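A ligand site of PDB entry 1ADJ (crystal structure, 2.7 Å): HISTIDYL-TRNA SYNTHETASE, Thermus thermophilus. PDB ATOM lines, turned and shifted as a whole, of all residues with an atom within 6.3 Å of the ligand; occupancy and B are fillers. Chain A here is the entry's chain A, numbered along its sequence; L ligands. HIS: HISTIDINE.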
ATOM      1  N   PRO A  80     -19.152  -2.298  19.354  1.00  0.00           N
ATOM      2  CA  PRO A  80     -19.662  -1.561  20.515  1.00  0.00           C
ATOM      3  C   PRO A  80     -20.890  -2.214  21.136  1.00  0.00           C
ATOM      4  O   PRO A  80     -21.285  -1.877  22.253  1.00  0.00           O
ATOM      5  CB  PRO A  80     -20.032  -0.213  19.906  1.00  0.00           C
ATOM      6  CG  PRO A  80     -20.593  -0.627  18.585  1.00  0.00           C
ATOM      7  CD  PRO A  80     -19.650  -1.713  18.099  1.00  0.00           C
ATOM      8  N   GLU A  81     -21.470  -3.166  20.416  1.00  0.00           N
ATOM      9  CA  GLU A  81     -22.671  -3.879  20.828  1.00  0.00           C
ATOM     10  C   GLU A  81     -22.795  -5.147  19.981  1.00  0.00           C
ATOM     11  O   GLU A  81     -22.247  -5.197  18.869  1.00  0.00           O
ATOM     12  CB  GLU A  81     -23.863  -2.924  20.668  1.00  0.00           C
ATOM     13  CG  GLU A  81     -25.194  -3.532  20.282  1.00  0.00           C
ATOM     14  CD  GLU A  81     -25.391  -3.634  18.783  1.00  0.00           C
ATOM     15  OE1 GLU A  81     -24.679  -2.955  18.012  1.00  0.00           O
ATOM     16  OE2 GLU A  81     -26.271  -4.405  18.370  1.00  0.00           O
ATOM     17  N   GLY A  82     -23.539  -6.140  20.464  1.00  0.00           N
ATOM     18  CA  GLY A  82     -23.658  -7.398  19.746  1.00  0.00           C
ATOM     19  C   GLY A  82     -24.761  -7.713  18.750  1.00  0.00           C
ATOM     20  O   GLY A  82     -24.543  -8.484  17.815  1.00  0.00           O
ATOM     21  N   THR A  83     -25.944  -7.116  18.917  1.00  0.00           N
ATOM     22  CA  THR A  83     -27.081  -7.401  18.041  1.00  0.00           C
ATOM     23  C   THR A  83     -26.847  -7.309  16.516  1.00  0.00           C
ATOM     24  O   THR A  83     -27.114  -8.261  15.779  1.00  0.00           O
ATOM     25  CB  THR A  83     -28.290  -6.528  18.419  1.00  0.00           C
ATOM     26  OG1 THR A  83     -28.416  -6.491  19.847  1.00  0.00           O
ATOM     27  CG2 THR A  83     -29.567  -7.075  17.805  1.00  0.00           C
ATOM     28  N   ALA A  84     -26.344  -6.169  16.056  1.00  0.00           N
ATOM     29  CA  ALA A  84     -26.086  -5.994  14.629  1.00  0.00           C
ATOM     30  C   ALA A  84     -25.167  -7.099  14.098  1.00  0.00           C
ATOM     31  O   ALA A  84     -25.462  -7.693  13.063  1.00  0.00           O
ATOM     32  CB  ALA A  84     -25.472  -4.617  14.368  1.00  0.00           C
ATOM     33  N   ARG A 112     -16.385   0.904  23.622  1.00  0.00           N
ATOM     34  CA  ARG A 112     -17.004   2.200  23.422  1.00  0.00           C
ATOM     35  C   ARG A 112     -16.063   3.349  23.760  1.00  0.00           C
ATOM     36  O   ARG A 112     -15.618   3.482  24.891  1.00  0.00           O
ATOM     37  CB  ARG A 112     -18.298   2.316  24.234  1.00  0.00           C
ATOM     38  CG  ARG A 112     -19.537   2.379  23.351  1.00  0.00           C
ATOM     39  CD  ARG A 112     -20.299   1.078  23.339  1.00  0.00           C
ATOM     40  NE  ARG A 112     -21.253   1.044  24.442  1.00  0.00           N
ATOM     41  CZ  ARG A 112     -22.507   0.629  24.340  1.00  0.00           C
ATOM     42  NH1 ARG A 112     -22.966   0.193  23.173  1.00  0.00           N
ATOM     43  NH2 ARG A 112     -23.319   0.684  25.383  1.00  0.00           N
ATOM     44  N   GLN A 126     -20.258  -8.194  27.973  1.00  0.00           N
ATOM     45  CA  GLN A 126     -21.677  -8.461  28.109  1.00  0.00           C
ATOM     46  C   GLN A 126     -22.107  -9.811  27.551  1.00  0.00           C
ATOM     47  O   GLN A 126     -21.415 -10.389  26.698  1.00  0.00           O
ATOM     48  CB  GLN A 126     -22.503  -7.331  27.472  1.00  0.00           C
ATOM     49  CG  GLN A 126     -22.528  -7.273  25.944  1.00  0.00           C
ATOM     50  CD  GLN A 126     -23.343  -6.090  25.428  1.00  0.00           C
ATOM     51  OE1 GLN A 126     -23.461  -5.057  26.094  1.00  0.00           O
ATOM     52  NE2 GLN A 126     -23.924  -6.244  24.231  1.00  0.00           N
ATOM     53  N   ASN A 128     -24.943 -11.676  25.593  1.00  0.00           N
ATOM     54  CA  ASN A 128     -25.901 -11.253  24.582  1.00  0.00           C
ATOM     55  C   ASN A 128     -26.757 -12.418  24.119  1.00  0.00           C
ATOM     56  O   ASN A 128     -26.230 -13.471  23.777  1.00  0.00           O
ATOM     57  CB  ASN A 128     -25.112 -10.659  23.413  1.00  0.00           C
ATOM     58  CG  ASN A 128     -25.992  -9.972  22.397  1.00  0.00           C
ATOM     59  OD1 ASN A 128     -26.200  -8.752  22.461  1.00  0.00           O
ATOM     60  ND2 ASN A 128     -26.439 -10.714  21.392  1.00  0.00           N
ATOM     61  N   TYR A 129     -28.083 -12.229  24.156  1.00  0.00           N
ATOM     62  CA  TYR A 129     -29.039 -13.246  23.722  1.00  0.00           C
ATOM     63  C   TYR A 129     -29.828 -12.673  22.554  1.00  0.00           C
ATOM     64  O   TYR A 129     -30.228 -11.513  22.575  1.00  0.00           O
ATOM     65  CB  TYR A 129     -30.000 -13.614  24.848  1.00  0.00           C
ATOM     66  CG  TYR A 129     -31.173 -14.451  24.384  1.00  0.00           C
ATOM     67  CD1 TYR A 129     -30.999 -15.789  24.024  1.00  0.00           C
ATOM     68  CD2 TYR A 129     -32.451 -13.901  24.273  1.00  0.00           C
ATOM     69  CE1 TYR A 129     -32.071 -16.558  23.585  1.00  0.00           C
ATOM     70  CE2 TYR A 129     -33.532 -14.661  23.828  1.00  0.00           C
ATOM     71  CZ  TYR A 129     -33.328 -15.999  23.489  1.00  0.00           C
ATOM     72  OH  TYR A 129     -34.380 -16.772  23.063  1.00  0.00           O
ATOM     73  N   GLU A 130     -30.170 -13.540  21.601  1.00  0.00           N
ATOM     74  CA  GLU A 130     -30.872 -13.127  20.401  1.00  0.00           C
ATOM     75  C   GLU A 130     -31.820 -14.224  19.913  1.00  0.00           C
ATOM     76  O   GLU A 130     -31.464 -15.406  19.889  1.00  0.00           O
ATOM     77  CB  GLU A 130     -29.818 -12.825  19.337  1.00  0.00           C
ATOM     78  CG  GLU A 130     -29.842 -11.452  18.701  1.00  0.00           C
ATOM     79  CD  GLU A 130     -29.803 -10.308  19.689  1.00  0.00           C
ATOM     80  OE1 GLU A 130     -30.892  -9.880  20.130  1.00  0.00           O
ATOM     81  OE2 GLU A 130     -28.712  -9.797  19.991  1.00  0.00           O
ATOM     82  N   ARG A 259     -34.526   3.544  24.499  1.00  0.00           N
ATOM     83  CA  ARG A 259     -33.361   2.693  24.610  1.00  0.00           C
ATOM     84  C   ARG A 259     -32.220   3.397  23.875  1.00  0.00           C
ATOM     85  O   ARG A 259     -32.456   4.366  23.153  1.00  0.00           O
ATOM     86  CB  ARG A 259     -33.654   1.320  24.013  1.00  0.00           C
ATOM     87  CG  ARG A 259     -32.834   0.224  24.626  1.00  0.00           C
ATOM     88  CD  ARG A 259     -33.302  -0.146  26.012  1.00  0.00           C
ATOM     89  NE  ARG A 259     -32.175  -0.615  26.822  1.00  0.00           N
ATOM     90  CZ  ARG A 259     -31.379  -1.640  26.511  1.00  0.00           C
ATOM     91  NH1 ARG A 259     -31.572  -2.346  25.395  1.00  0.00           N
ATOM     92  NH2 ARG A 259     -30.361  -1.952  27.294  1.00  0.00           N
ATOM     93  N   LEU A 261     -30.418   2.582  21.286  1.00  0.00           N
ATOM     94  CA  LEU A 261     -30.181   2.251  19.886  1.00  0.00           C
ATOM     95  C   LEU A 261     -31.418   2.528  19.020  1.00  0.00           C
ATOM     96  O   LEU A 261     -32.539   2.442  19.509  1.00  0.00           O
ATOM     97  CB  LEU A 261     -29.736   0.790  19.756  1.00  0.00           C
ATOM     98  CG  LEU A 261     -28.559   0.428  20.667  1.00  0.00           C
ATOM     99  CD1 LEU A 261     -29.048  -0.007  22.029  1.00  0.00           C
ATOM    100  CD2 LEU A 261     -27.743  -0.670  20.044  1.00  0.00           C
ATOM    101  N   TYR A 263     -32.400   0.819  16.100  1.00  0.00           N
ATOM    102  CA  TYR A 263     -33.006  -0.321  15.410  1.00  0.00           C
ATOM    103  C   TYR A 263     -34.226  -0.937  16.115  1.00  0.00           C
ATOM    104  O   TYR A 263     -34.910  -1.795  15.552  1.00  0.00           O
ATOM    105  CB  TYR A 263     -31.946  -1.411  15.137  1.00  0.00           C
ATOM    106  CG  TYR A 263     -31.209  -1.932  16.349  1.00  0.00           C
ATOM    107  CD1 TYR A 263     -31.893  -2.352  17.500  1.00  0.00           C
ATOM    108  CD2 TYR A 263     -29.820  -2.043  16.359  1.00  0.00           C
ATOM    109  CE1 TYR A 263     -31.229  -2.866  18.593  1.00  0.00           C
ATOM    110  CE2 TYR A 263     -29.135  -2.553  17.444  1.00  0.00           C
ATOM    111  CZ  TYR A 263     -29.850  -2.970  18.561  1.00  0.00           C
ATOM    112  OH  TYR A 263     -29.181  -3.520  19.641  1.00  0.00           O
ATOM    113  N   TYR A 264     -34.483  -0.500  17.352  1.00  0.00           N
ATOM    114  CA  TYR A 264     -35.592  -0.994  18.153  1.00  0.00           C
ATOM    115  C   TYR A 264     -36.974  -0.658  17.625  1.00  0.00           C
ATOM    116  O   TYR A 264     -37.239   0.465  17.219  1.00  0.00           O
ATOM    117  CB  TYR A 264     -35.491  -0.493  19.582  1.00  0.00           C
ATOM    118  CG  TYR A 264     -34.469  -1.210  20.414  1.00  0.00           C
ATOM    119  CD1 TYR A 264     -34.501  -2.598  20.556  1.00  0.00           C
ATOM    120  CD2 TYR A 264     -33.471  -0.506  21.074  1.00  0.00           C
ATOM    121  CE1 TYR A 264     -33.572  -3.251  21.340  1.00  0.00           C
ATOM    122  CE2 TYR A 264     -32.540  -1.144  21.846  1.00  0.00           C
ATOM    123  CZ  TYR A 264     -32.591  -2.520  21.983  1.00  0.00           C
ATOM    124  OH  TYR A 264     -31.657  -3.140  22.779  1.00  0.00           O
ATOM    125  N   GLY A 284     -30.599  -4.946  29.376  1.00  0.00           N
ATOM    126  CA  GLY A 284     -31.848  -4.647  28.721  1.00  0.00           C
ATOM    127  C   GLY A 284     -31.885  -5.206  27.325  1.00  0.00           C
ATOM    128  O   GLY A 284     -30.990  -5.936  26.920  1.00  0.00           O
ATOM    129  N   GLY A 285     -32.938  -4.866  26.589  1.00  0.00           N
ATOM    130  CA  GLY A 285     -33.087  -5.364  25.239  1.00  0.00           C
ATOM    131  C   GLY A 285     -34.432  -4.977  24.669  1.00  0.00           C
ATOM    132  O   GLY A 285     -35.125  -4.134  25.239  1.00  0.00           O
ATOM    133  N   GLY A 286     -34.796  -5.608  23.558  1.00  0.00           N
ATOM    134  CA  GLY A 286     -36.054  -5.309  22.917  1.00  0.00           C
ATOM    135  C   GLY A 286     -36.139  -5.914  21.536  1.00  0.00           C
ATOM    136  O   GLY A 286     -35.236  -6.657  21.115  1.00  0.00           O
ATOM    137  N   ARG A 287     -37.218  -5.617  20.823  1.00  0.00           N
ATOM    138  CA  ARG A 287     -37.411  -6.147  19.490  1.00  0.00           C
ATOM    139  C   ARG A 287     -36.740  -5.212  18.484  1.00  0.00           C
ATOM    140  O   ARG A 287     -36.554  -4.031  18.762  1.00  0.00           O
ATOM    141  CB  ARG A 287     -38.906  -6.302  19.228  1.00  0.00           C
ATOM    142  CG  ARG A 287     -39.243  -6.997  17.936  1.00  0.00           C
ATOM    143  CD  ARG A 287     -40.669  -7.507  17.965  1.00  0.00           C
ATOM    144  NE  ARG A 287     -40.784  -8.850  18.535  1.00  0.00           N
ATOM    145  CZ  ARG A 287     -40.464  -9.956  17.872  1.00  0.00           C
ATOM    146  NH1 ARG A 287     -40.002  -9.873  16.623  1.00  0.00           N
ATOM    147  NH2 ARG A 287     -40.688 -11.135  18.410  1.00  0.00           N
ATOM    148  N   TYR A 288     -36.363  -5.743  17.326  1.00  0.00           N
ATOM    149  CA  TYR A 288     -35.679  -4.934  16.324  1.00  0.00           C
ATOM    150  C   TYR A 288     -35.853  -5.454  14.906  1.00  0.00           C
ATOM    151  O   TYR A 288     -34.895  -5.753  14.198  1.00  0.00           O
ATOM    152  CB  TYR A 288     -34.172  -4.851  16.675  1.00  0.00           C
ATOM    153  CG  TYR A 288     -33.550  -6.205  16.917  1.00  0.00           C
ATOM    154  CD1 TYR A 288     -33.128  -7.008  15.854  1.00  0.00           C
ATOM    155  CD2 TYR A 288     -33.446  -6.724  18.213  1.00  0.00           C
ATOM    156  CE1 TYR A 288     -32.638  -8.286  16.058  1.00  0.00           C
ATOM    157  CE2 TYR A 288     -32.957  -8.012  18.437  1.00  0.00           C
ATOM    158  CZ  TYR A 288     -32.561  -8.780  17.351  1.00  0.00           C
ATOM    159  OH  TYR A 288     -32.123 -10.070  17.546  1.00  0.00           O
ATOM    160  N   VAL A 303     -35.725 -10.391  18.675  1.00  0.00           N
ATOM    161  CA  VAL A 303     -35.777  -9.818  20.009  1.00  0.00           C
ATOM    162  C   VAL A 303     -34.553 -10.366  20.714  1.00  0.00           C
ATOM    163  O   VAL A 303     -34.047 -11.428  20.356  1.00  0.00           O
ATOM    164  CB  VAL A 303     -36.975 -10.308  20.869  1.00  0.00           C
ATOM    165  CG1 VAL A 303     -37.764  -9.133  21.381  1.00  0.00           C
ATOM    166  CG2 VAL A 303     -37.817 -11.321  20.142  1.00  0.00           C
ATOM    167  N   GLY A 304     -34.124  -9.692  21.760  1.00  0.00           N
ATOM    168  CA  GLY A 304     -32.991 -10.182  22.509  1.00  0.00           C
ATOM    169  C   GLY A 304     -32.661  -9.223  23.632  1.00  0.00           C
ATOM    170  O   GLY A 304     -33.386  -8.255  23.864  1.00  0.00           O
ATOM    171  N   PHE A 305     -31.570  -9.496  24.314  1.00  0.00           N
ATOM    172  CA  PHE A 305     -31.135  -8.640  25.399  1.00  0.00           C
ATOM    173  C   PHE A 305     -29.638  -8.803  25.558  1.00  0.00           C
ATOM    174  O   PHE A 305     -29.015  -9.617  24.864  1.00  0.00           O
ATOM    175  CB  PHE A 305     -31.838  -9.007  26.702  1.00  0.00           C
ATOM    176  CG  PHE A 305     -31.459 -10.351  27.232  1.00  0.00           C
ATOM    177  CD1 PHE A 305     -30.328 -10.511  28.037  1.00  0.00           C
ATOM    178  CD2 PHE A 305     -32.232 -11.470  26.961  1.00  0.00           C
ATOM    179  CE1 PHE A 305     -29.975 -11.755  28.547  1.00  0.00           C
ATOM    180  CE2 PHE A 305     -31.892 -12.726  27.469  1.00  0.00           C
ATOM    181  CZ  PHE A 305     -30.768 -12.868  28.263  1.00  0.00           C
ATOM    182  N   ALA A 306     -29.069  -8.036  26.466  1.00  0.00           N
ATOM    183  CA  ALA A 306     -27.645  -8.099  26.761  1.00  0.00           C
ATOM    184  C   ALA A 306     -27.499  -7.487  28.127  1.00  0.00           C
ATOM    185  O   ALA A 306     -28.309  -6.653  28.519  1.00  0.00           O
ATOM    186  CB  ALA A 306     -26.860  -7.288  25.744  1.00  0.00           C
HETATM  187  N   HIS L   1     -27.720  -4.633  21.570  1.00  0.00           N
HETATM  188  CA  HIS L   1     -28.392  -4.274  22.820  1.00  0.00           C
HETATM  189  C   HIS L   1     -27.470  -3.521  23.766  1.00  0.00           C
HETATM  190  O   HIS L   1     -26.315  -3.279  23.371  1.00  0.00           O
HETATM  191  CB  HIS L   1     -28.975  -5.520  23.493  1.00  0.00           C
HETATM  192  CG  HIS L   1     -30.016  -6.216  22.671  1.00  0.00           C
HETATM  193  ND1 HIS L   1     -31.069  -5.547  22.104  1.00  0.00           N
HETATM  194  CD2 HIS L   1     -30.121  -7.507  22.263  1.00  0.00           C
HETATM  195  CE1 HIS L   1     -31.794  -6.383  21.380  1.00  0.00           C
HETATM  196  NE2 HIS L   1     -31.235  -7.582  21.466  1.00  0.00           N
HETATM  197  OXT HIS L   1     -27.912  -3.154  24.880  1.00  0.00           O
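The side-chain hydroxyl (OG1) of Thr 83 sits at hydrogen-bond distance from a nitrogen (N) of the ligand (2.6 Å). The backbone NH of Phe 305 sits close to a nitrogen (NE2) of the ligand (3.4 Å). The guanidinium group (NH2) of Arg 259 lies within salt-bridge range of an oxygen (OXT) of the ligand, at 3.6 Å. O of Gly 304 lies close to NE2 of the ligand, 3.3 Å away. OE1 of Glu 130 lies within hydrogen-bond range of NE2 of the ligand (2.7 Å). OH of Tyr 263 is in hydrogen-bond range of N of the ligand (2.7 Å). The side-chain carboxylate (OE2) of Glu 81 is in salt-bridge range of a nitrogen (N) of the ligand (3.5 Å). ND1 of the ligand is in hydrogen-bond range of OH of Tyr 264 (2.6 Å).
OH of Tyr 264 sits at hydrogen-bond distance from NH1 of Arg 259 (2.7 Å). The side-chain carboxylate (OE2) of Glu 130 sits at hydrogen-bond distance from the side-chain hydroxyl (OG1) of Thr 83 (3.3 Å). The backbone NH (N) of Thr 83 lies within hydrogen-bond range of the side-chain carboxylate (OE2) of Glu 81, 2.8 Å away. The side-chain carboxylate (OE2) of Glu 81 lies within hydrogen-bond range of the backbone NH (N) of Ala 84, 2.9 Å away. N of Tyr 129 is in hydrogen-bond range of O of Phe 305 (2.9 Å). OH of Tyr 288 lies within hydrogen-bond range of OE1 of Glu 130, at 2.9 Å. The backbone carbonyl oxygen of Gly 304 is in hydrogen-bond range of the backbone NH of Gly 286 (3.0 Å). O of Gly 284 lies within hydrogen-bond range of N of Ala 306 (2.9 Å).
Gln 126 touches the ligand. O of Gly 284 touches CB of the ligand (3.997 Å). CA of Gly 285 touches ND1 of the ligand, at 3.7 Å. O of Gly 286 touches CE1 of the ligand (3.5 Å). Tyr 288 touches the ligand (CE2 to NE2, 3.5 Å). Ala 306 touches the ligand. Hydrophobic or aromatic side chains that line the ligand: Tyr 264, Tyr 288 and Ala 306. Of the 23 residues printed, 14 come within 4 Å of the ligand. The nearest printed residue that does not touch the ligand is Tyr 129 (4.02 Å).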
